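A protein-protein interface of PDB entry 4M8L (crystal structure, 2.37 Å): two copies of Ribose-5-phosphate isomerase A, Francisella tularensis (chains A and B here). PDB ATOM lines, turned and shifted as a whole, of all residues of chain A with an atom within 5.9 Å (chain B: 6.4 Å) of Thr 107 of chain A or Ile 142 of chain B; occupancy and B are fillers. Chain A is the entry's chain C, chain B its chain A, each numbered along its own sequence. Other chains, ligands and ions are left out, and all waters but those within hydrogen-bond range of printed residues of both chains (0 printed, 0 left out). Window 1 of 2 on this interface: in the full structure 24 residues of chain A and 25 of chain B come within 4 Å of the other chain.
The side-chain carboxylate (OE2) of Glu 140 of chain A sits at hydrogen-bond distance from the side-chain amide nitrogen (ND2) of Asn 170 of chain A, 3.2 Å away.
The side-chain hydroxyl of Thr 107 of chain A is in hydrogen-bond range of the side-chain hydroxyl of Thr 200 of chain A, at 2.9 Å.
The backbone carbonyl oxygen (O) of Arg 108 of chain A is in hydrogen-bond range of the side-chain sulfur (SG) of Cys 112 of chain A (3.3 Å).
The backbone carbonyl oxygen (O) of Gly 197 of chain B is in hydrogen-bond range of the backbone NH (N) of Ile 142 of chain B.
The guanidinium group (NE) of Arg 108 of chain A sits at hydrogen-bond distance from the side-chain amide oxygen (OD1) of Asn 170 of chain A.
The side-chain carboxylate (OE1) of Glu 140 of chain A lies within hydrogen-bond range of the side-chain hydroxyl (OG1) of Thr 107 of chain A (2.4 Å).
3 positions are printed for both chains.
Among the printed residues, merely in contact across the chains: Thr 107 of chain A with Ile 142 of chain B, Arg 108 of chain A with Met 144 of chain B, Lys 110 of chain A with Thr 196 of chain B, Ile 111 of chain A with Ile 142 of chain B, Ile 111 of chain A with Ala 145 of chain B, Ile 111 of chain A with Thr 196 of chain B, Ile 111 of chain A with Gly 197 of chain B, Cys 112 of chain A with Met 144 of chain B and Asn 170 of chain A with Ile 142 of chain B.
Thr 107 of chain A touches just one residue of chain B: Ile 142.
Of the printed residues of chain B, Cys 112 of chain A touches Met 144.
Asn 172 of chain A touches none of the printed residues of chain B.
Ile 142 of chain B touches just these residues of chain A: Thr 107, Ile 111 and Asn 170.
Of the printed residues of chain A, Ala 145 of chain B touches Ile 111 (3.5 Å).
The nearest printed residue of chain A that does not touch Met 144 of chain B is Ile 111 of chain A (4.4 Å).
Of the 14 printed residues of chain B, 5 touch a printed residue of chain A.
Hydrophobic or aromatic side chains of chain B within 4 Å of the printed part of chain A: Ile 142, Met 144 and Ala 145.
Among the printed residues, 9 pairs touch across the chains.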
ATOM      1  N   ALA A 104     -25.338  19.670  -7.041  1.00  0.00           N
ATOM      2  CA  ALA A 104     -24.796  20.949  -7.544  1.00  0.00           C
ATOM      3  C   ALA A 104     -23.847  20.899  -8.758  1.00  0.00           C
ATOM      4  O   ALA A 104     -23.489  21.954  -9.283  1.00  0.00           O
ATOM      5  CB  ALA A 104     -24.134  21.724  -6.401  1.00  0.00           C
ATOM      6  N   ALA A 105     -23.471  19.708  -9.230  1.00  0.00           N
ATOM      7  CA  ALA A 105     -22.475  19.578 -10.319  1.00  0.00           C
ATOM      8  C   ALA A 105     -23.115  19.527 -11.707  1.00  0.00           C
ATOM      9  O   ALA A 105     -22.490  19.066 -12.661  1.00  0.00           O
ATOM     10  CB  ALA A 105     -21.609  18.339 -10.108  1.00  0.00           C
ATOM     11  N   LEU A 106     -24.340  20.027 -11.831  1.00  0.00           N
ATOM     12  CA  LEU A 106     -25.154  19.782 -13.019  1.00  0.00           C
ATOM     13  C   LEU A 106     -24.578  20.358 -14.317  1.00  0.00           C
ATOM     14  O   LEU A 106     -24.792  19.795 -15.391  1.00  0.00           O
ATOM     15  CB  LEU A 106     -26.588  20.279 -12.787  1.00  0.00           C
ATOM     16  CG  LEU A 106     -26.920  21.760 -12.989  1.00  0.00           C
ATOM     17  CD1 LEU A 106     -27.873  21.902 -14.161  1.00  0.00           C
ATOM     18  CD2 LEU A 106     -27.554  22.370 -11.750  1.00  0.00           C
ATOM     19  N   THR A 107     -23.852  21.468 -14.229  1.00  0.00           N
ATOM     20  CA  THR A 107     -23.278  22.088 -15.422  1.00  0.00           C
ATOM     21  C   THR A 107     -22.227  21.180 -16.058  1.00  0.00           C
ATOM     22  O   THR A 107     -22.341  20.806 -17.224  1.00  0.00           O
ATOM     23  CB  THR A 107     -22.667  23.470 -15.113  1.00  0.00           C
ATOM     24  OG1 THR A 107     -23.726  24.401 -14.850  1.00  0.00           O
ATOM     25  CG2 THR A 107     -21.848  23.985 -16.290  1.00  0.00           C
ATOM     26  N   ARG A 108     -21.218  20.815 -15.279  1.00  0.00           N
ATOM     27  CA  ARG A 108     -20.144  19.966 -15.782  1.00  0.00           C
ATOM     28  C   ARG A 108     -20.625  18.547 -16.086  1.00  0.00           C
ATOM     29  O   ARG A 108     -20.085  17.882 -16.974  1.00  0.00           O
ATOM     30  CB  ARG A 108     -18.995  19.935 -14.787  1.00  0.00           C
ATOM     31  CG  ARG A 108     -18.333  21.286 -14.595  1.00  0.00           C
ATOM     32  CD  ARG A 108     -17.093  21.171 -13.729  1.00  0.00           C
ATOM     33  NE  ARG A 108     -16.478  22.472 -13.469  1.00  0.00           N
ATOM     34  CZ  ARG A 108     -15.320  22.644 -12.836  1.00  0.00           C
ATOM     35  NH1 ARG A 108     -14.632  21.595 -12.392  1.00  0.00           N
ATOM     36  NH2 ARG A 108     -14.846  23.871 -12.648  1.00  0.00           N
ATOM     37  N   GLU A 109     -21.644  18.097 -15.356  1.00  0.00           N
ATOM     38  CA  GLU A 109     -22.284  16.812 -15.639  1.00  0.00           C
ATOM     39  C   GLU A 109     -22.941  16.821 -17.013  1.00  0.00           C
ATOM     40  O   GLU A 109     -22.866  15.839 -17.739  1.00  0.00           O
ATOM     41  CB  GLU A 109     -23.331  16.479 -14.575  1.00  0.00           C
ATOM     42  CG  GLU A 109     -22.731  15.977 -13.271  1.00  0.00           C
ATOM     43  CD  GLU A 109     -23.759  15.749 -12.177  1.00  0.00           C
ATOM     44  OE1 GLU A 109     -23.583  14.776 -11.426  1.00  0.00           O
ATOM     45  OE2 GLU A 109     -24.740  16.512 -12.061  1.00  0.00           O
ATOM     46  N   LYS A 110     -23.569  17.936 -17.370  1.00  0.00           N
ATOM     47  CA  LYS A 110     -24.244  18.056 -18.659  1.00  0.00           C
ATOM     48  C   LYS A 110     -23.231  18.184 -19.798  1.00  0.00           C
ATOM     49  O   LYS A 110     -23.440  17.649 -20.887  1.00  0.00           O
ATOM     50  CB  LYS A 110     -25.204  19.250 -18.651  1.00  0.00           C
ATOM     51  CG  LYS A 110     -26.341  19.146 -19.655  1.00  0.00           C
ATOM     52  CD  LYS A 110     -27.445  20.146 -19.331  1.00  0.00           C
ATOM     53  CE  LYS A 110     -28.799  19.688 -19.844  1.00  0.00           C
ATOM     54  NZ  LYS A 110     -29.906  20.508 -19.285  1.00  0.00           N
ATOM     55  N   ILE A 111     -22.141  18.902 -19.537  1.00  0.00           N
ATOM     56  CA  ILE A 111     -21.041  19.034 -20.496  1.00  0.00           C
ATOM     57  C   ILE A 111     -20.412  17.660 -20.770  1.00  0.00           C
ATOM     58  O   ILE A 111     -20.169  17.308 -21.919  1.00  0.00           O
ATOM     59  CB  ILE A 111     -19.968  20.024 -19.990  1.00  0.00           C
ATOM     60  CG1 ILE A 111     -20.536  21.449 -19.941  1.00  0.00           C
ATOM     61  CG2 ILE A 111     -18.736  19.996 -20.891  1.00  0.00           C
ATOM     62  CD1 ILE A 111     -19.779  22.390 -19.021  1.00  0.00           C
ATOM     63  N   CYS A 112     -20.169  16.890 -19.712  1.00  0.00           N
ATOM     64  CA  CYS A 112     -19.628  15.533 -19.857  1.00  0.00           C
ATOM     65  C   CYS A 112     -20.544  14.625 -20.672  1.00  0.00           C
ATOM     66  O   CYS A 112     -20.068  13.868 -21.520  1.00  0.00           O
ATOM     67  CB  CYS A 112     -19.367  14.899 -18.491  1.00  0.00           C
ATOM     68  SG  CYS A 112     -17.912  15.554 -17.651  1.00  0.00           S
ATOM     69  N   GLU A 140     -28.809  26.215 -12.423  1.00  0.00           N
ATOM     70  CA  GLU A 140     -27.612  26.995 -12.115  1.00  0.00           C
ATOM     71  C   GLU A 140     -27.712  28.339 -12.822  1.00  0.00           C
ATOM     72  O   GLU A 140     -27.890  28.387 -14.040  1.00  0.00           O
ATOM     73  CB  GLU A 140     -26.341  26.250 -12.541  1.00  0.00           C
ATOM     74  CG  GLU A 140     -25.046  26.929 -12.098  1.00  0.00           C
ATOM     75  CD  GLU A 140     -23.809  26.057 -12.269  1.00  0.00           C
ATOM     76  OE1 GLU A 140     -23.951  24.834 -12.473  1.00  0.00           O
ATOM     77  OE2 GLU A 140     -22.682  26.592 -12.193  1.00  0.00           O
ATOM     78  N   ASN A 170     -18.280  26.370 -10.657  1.00  0.00           N
ATOM     79  CA  ASN A 170     -18.160  27.427 -11.664  1.00  0.00           C
ATOM     80  C   ASN A 170     -18.434  28.840 -11.143  1.00  0.00           C
ATOM     81  O   ASN A 170     -18.486  29.790 -11.928  1.00  0.00           O
ATOM     82  CB  ASN A 170     -19.116  27.120 -12.820  1.00  0.00           C
ATOM     83  CG  ASN A 170     -19.036  25.670 -13.262  1.00  0.00           C
ATOM     84  OD1 ASN A 170     -18.003  25.212 -13.739  1.00  0.00           O
ATOM     85  ND2 ASN A 170     -20.129  24.928 -13.063  1.00  0.00           N
ATOM     86  N   ASN A 172     -21.206  29.908  -9.522  1.00  0.00           N
ATOM     87  CA  ASN A 172     -22.607  30.286  -9.660  1.00  0.00           C
ATOM     88  C   ASN A 172     -23.455  29.793  -8.498  1.00  0.00           C
ATOM     89  O   ASN A 172     -22.967  29.072  -7.630  1.00  0.00           O
ATOM     90  CB  ASN A 172     -23.159  29.738 -10.972  1.00  0.00           C
ATOM     91  CG  ASN A 172     -22.450  30.312 -12.185  1.00  0.00           C
ATOM     92  OD1 ASN A 172     -22.205  31.519 -12.259  1.00  0.00           O
ATOM     93  ND2 ASN A 172     -22.099  29.452 -13.127  1.00  0.00           N
ATOM     94  N   VAL A 199     -27.352  29.319 -16.590  1.00  0.00           N
ATOM     95  CA  VAL A 199     -26.168  28.641 -17.095  1.00  0.00           C
ATOM     96  C   VAL A 199     -26.590  27.269 -17.596  1.00  0.00           C
ATOM     97  O   VAL A 199     -26.427  26.948 -18.772  1.00  0.00           O
ATOM     98  CB  VAL A 199     -25.088  28.512 -16.001  1.00  0.00           C
ATOM     99  CG1 VAL A 199     -23.885  27.731 -16.512  1.00  0.00           C
ATOM    100  CG2 VAL A 199     -24.661  29.893 -15.525  1.00  0.00           C
ATOM    101  N   THR A 200     -27.147  26.471 -16.687  1.00  0.00           N
ATOM    102  CA  THR A 200     -27.647  25.143 -17.008  1.00  0.00           C
ATOM    103  C   THR A 200     -28.895  24.871 -16.175  1.00  0.00           C
ATOM    104  O   THR A 200     -29.002  25.348 -15.044  1.00  0.00           O
ATOM    105  CB  THR A 200     -26.579  24.061 -16.714  1.00  0.00           C
ATOM    106  OG1 THR A 200     -25.321  24.455 -17.267  1.00  0.00           O
ATOM    107  CG2 THR A 200     -26.963  22.734 -17.322  1.00  0.00           C
ATOM    108  N   GLU B 140     -19.385  33.399 -24.515  1.00  0.00           N
ATOM    109  CA  GLU B 140     -18.846  33.082 -23.193  1.00  0.00           C
ATOM    110  C   GLU B 140     -19.179  31.639 -22.860  1.00  0.00           C
ATOM    111  O   GLU B 140     -20.348  31.243 -22.907  1.00  0.00           O
ATOM    112  CB  GLU B 140     -19.408  34.020 -22.122  1.00  0.00           C
ATOM    113  CG  GLU B 140     -18.763  33.851 -20.748  1.00  0.00           C
ATOM    114  CD  GLU B 140     -19.118  34.959 -19.769  1.00  0.00           C
ATOM    115  OE1 GLU B 140     -19.634  36.005 -20.203  1.00  0.00           O
ATOM    116  OE2 GLU B 140     -18.866  34.792 -18.559  1.00  0.00           O
ATOM    117  N   VAL B 141     -18.150  30.852 -22.539  1.00  0.00           N
ATOM    118  CA  VAL B 141     -18.322  29.415 -22.315  1.00  0.00           C
ATOM    119  C   VAL B 141     -17.699  28.965 -21.000  1.00  0.00           C
ATOM    120  O   VAL B 141     -16.747  29.568 -20.511  1.00  0.00           O
ATOM    121  CB  VAL B 141     -17.722  28.570 -23.467  1.00  0.00           C
ATOM    122  CG1 VAL B 141     -18.336  28.962 -24.799  1.00  0.00           C
ATOM    123  CG2 VAL B 141     -16.209  28.703 -23.525  1.00  0.00           C
ATOM    124  N   ILE B 142     -18.242  27.888 -20.449  1.00  0.00           N
ATOM    125  CA  ILE B 142     -17.681  27.251 -19.267  1.00  0.00           C
ATOM    126  C   ILE B 142     -16.332  26.660 -19.678  1.00  0.00           C
ATOM    127  O   ILE B 142     -16.267  25.931 -20.673  1.00  0.00           O
ATOM    128  CB  ILE B 142     -18.633  26.154 -18.736  1.00  0.00           C
ATOM    129  CG1 ILE B 142     -19.931  26.779 -18.194  1.00  0.00           C
ATOM    130  CG2 ILE B 142     -17.943  25.284 -17.684  1.00  0.00           C
ATOM    131  CD1 ILE B 142     -19.768  27.524 -16.884  1.00  0.00           C
ATOM    132  N   PRO B 143     -15.252  26.991 -18.937  1.00  0.00           N
ATOM    133  CA  PRO B 143     -13.895  26.575 -19.334  1.00  0.00           C
ATOM    134  C   PRO B 143     -13.777  25.100 -19.720  1.00  0.00           C
ATOM    135  O   PRO B 143     -13.170  24.777 -20.735  1.00  0.00           O
ATOM    136  CB  PRO B 143     -13.049  26.878 -18.086  1.00  0.00           C
ATOM    137  CG  PRO B 143     -13.777  27.983 -17.399  1.00  0.00           C
ATOM    138  CD  PRO B 143     -15.241  27.755 -17.673  1.00  0.00           C
ATOM    139  N   MET B 144     -14.382  24.226 -18.925  1.00  0.00           N
ATOM    140  CA  MET B 144     -14.369  22.786 -19.179  1.00  0.00           C
ATOM    141  C   MET B 144     -14.952  22.382 -20.544  1.00  0.00           C
ATOM    142  O   MET B 144     -14.563  21.357 -21.104  1.00  0.00           O
ATOM    143  CB  MET B 144     -15.142  22.070 -18.064  1.00  0.00           C
ATOM    144  CG  MET B 144     -15.243  20.564 -18.231  1.00  0.00           C
ATOM    145  SD  MET B 144     -16.193  19.794 -16.918  1.00  0.00           S
ATOM    146  CE  MET B 144     -15.897  18.074 -17.294  1.00  0.00           C
ATOM    147  N   ALA B 145     -15.886  23.175 -21.068  1.00  0.00           N
ATOM    148  CA  ALA B 145     -16.601  22.829 -22.300  1.00  0.00           C
ATOM    149  C   ALA B 145     -16.004  23.471 -23.545  1.00  0.00           C
ATOM    150  O   ALA B 145     -16.564  23.335 -24.634  1.00  0.00           O
ATOM    151  CB  ALA B 145     -18.069  23.221 -22.176  1.00  0.00           C
ATOM    152  N   ARG B 146     -14.868  24.147 -23.400  1.00  0.00           N
ATOM    153  CA  ARG B 146     -14.312  24.941 -24.498  1.00  0.00           C
ATOM    154  C   ARG B 146     -14.056  24.111 -25.760  1.00  0.00           C
ATOM    155  O   ARG B 146     -14.470  24.493 -26.855  1.00  0.00           O
ATOM    156  CB  ARG B 146     -13.027  25.642 -24.054  1.00  0.00           C
ATOM    157  CG  ARG B 146     -12.456  26.591 -25.095  1.00  0.00           C
ATOM    158  CD  ARG B 146     -11.352  27.451 -24.504  1.00  0.00           C
ATOM    159  NE  ARG B 146     -10.228  26.633 -24.049  1.00  0.00           N
ATOM    160  CZ  ARG B 146      -9.290  26.124 -24.843  1.00  0.00           C
ATOM    161  NH1 ARG B 146      -9.310  26.343 -26.156  1.00  0.00           N
ATOM    162  NH2 ARG B 146      -8.318  25.388 -24.320  1.00  0.00           N
ATOM    163  N   ILE B 149     -17.381  22.751 -27.321  1.00  0.00           N
ATOM    164  CA  ILE B 149     -18.132  23.820 -27.977  1.00  0.00           C
ATOM    165  C   ILE B 149     -17.439  24.273 -29.254  1.00  0.00           C
ATOM    166  O   ILE B 149     -18.102  24.537 -30.262  1.00  0.00           O
ATOM    167  CB  ILE B 149     -18.344  25.019 -27.029  1.00  0.00           C
ATOM    168  CG1 ILE B 149     -19.295  24.620 -25.900  1.00  0.00           C
ATOM    169  CG2 ILE B 149     -18.910  26.221 -27.778  1.00  0.00           C
ATOM    170  CD1 ILE B 149     -19.263  25.561 -24.715  1.00  0.00           C
ATOM    171  N   ASN B 172     -15.354  32.772 -16.554  1.00  0.00           N
ATOM    172  CA  ASN B 172     -15.441  31.998 -17.782  1.00  0.00           C
ATOM    173  C   ASN B 172     -14.475  32.504 -18.838  1.00  0.00           C
ATOM    174  O   ASN B 172     -13.817  33.520 -18.646  1.00  0.00           O
ATOM    175  CB  ASN B 172     -16.871  32.040 -18.316  1.00  0.00           C
ATOM    176  CG  ASN B 172     -17.862  31.412 -17.354  1.00  0.00           C
ATOM    177  OD1 ASN B 172     -17.617  30.333 -16.809  1.00  0.00           O
ATOM    178  ND2 ASN B 172     -18.991  32.076 -17.147  1.00  0.00           N
ATOM    179  N   VAL B 173     -14.401  31.775 -19.948  1.00  0.00           N
ATOM    180  CA  VAL B 173     -13.556  32.148 -21.083  1.00  0.00           C
ATOM    181  C   VAL B 173     -14.412  32.499 -22.298  1.00  0.00           C
ATOM    182  O   VAL B 173     -15.595  32.148 -22.361  1.00  0.00           O
ATOM    183  CB  VAL B 173     -12.549  31.030 -21.450  1.00  0.00           C
ATOM    184  CG1 VAL B 173     -11.527  30.851 -20.337  1.00  0.00           C
ATOM    185  CG2 VAL B 173     -13.252  29.710 -21.741  1.00  0.00           C
ATOM    186  N   THR B 196     -24.616  23.027 -25.060  1.00  0.00           N
ATOM    187  CA  THR B 196     -24.234  22.790 -23.672  1.00  0.00           C
ATOM    188  C   THR B 196     -22.873  23.413 -23.361  1.00  0.00           C
ATOM    189  O   THR B 196     -21.921  23.253 -24.125  1.00  0.00           O
ATOM    190  CB  THR B 196     -24.164  21.280 -23.369  1.00  0.00           C
ATOM    191  OG1 THR B 196     -25.328  20.630 -23.900  1.00  0.00           O
ATOM    192  CG2 THR B 196     -24.081  21.028 -21.869  1.00  0.00           C
ATOM    193  N   GLY B 197     -22.798  24.117 -22.232  1.00  0.00           N
ATOM    194  CA  GLY B 197     -21.579  24.801 -21.817  1.00  0.00           C
ATOM    195  C   GLY B 197     -21.499  26.262 -22.230  1.00  0.00           C
ATOM    196  O   GLY B 197     -20.622  26.986 -21.748  1.00  0.00           O
ATOM    197  N   VAL B 198     -22.381  26.705 -23.128  1.00  0.00           N
ATOM    198  CA  VAL B 198     -22.432  28.116 -23.507  1.00  0.00           C
ATOM    199  C   VAL B 198     -23.189  28.879 -22.422  1.00  0.00           C
ATOM    200  O   VAL B 198     -24.320  28.536 -22.090  1.00  0.00           O
ATOM    201  CB  VAL B 198     -23.123  28.350 -24.869  1.00  0.00           C
ATOM    202  CG1 VAL B 198     -23.221  29.840 -25.175  1.00  0.00           C
ATOM    203  CG2 VAL B 198     -22.366  27.649 -25.985  1.00  0.00           C
ATOM    204  N   VAL B 199     -22.551  29.908 -21.876  1.00  0.00           N
ATOM    205  CA  VAL B 199     -23.171  30.745 -20.866  1.00  0.00           C
ATOM    206  C   VAL B 199     -24.026  31.788 -21.577  1.00  0.00           C
ATOM    207  O   VAL B 199     -25.245  31.839 -21.390  1.00  0.00           O
ATOM    208  CB  VAL B 199     -22.112  31.425 -19.979  1.00  0.00           C
ATOM    209  CG1 VAL B 199     -22.775  32.354 -18.972  1.00  0.00           C
ATOM    210  CG2 VAL B 199     -21.279  30.373 -19.261  1.00  0.00           C
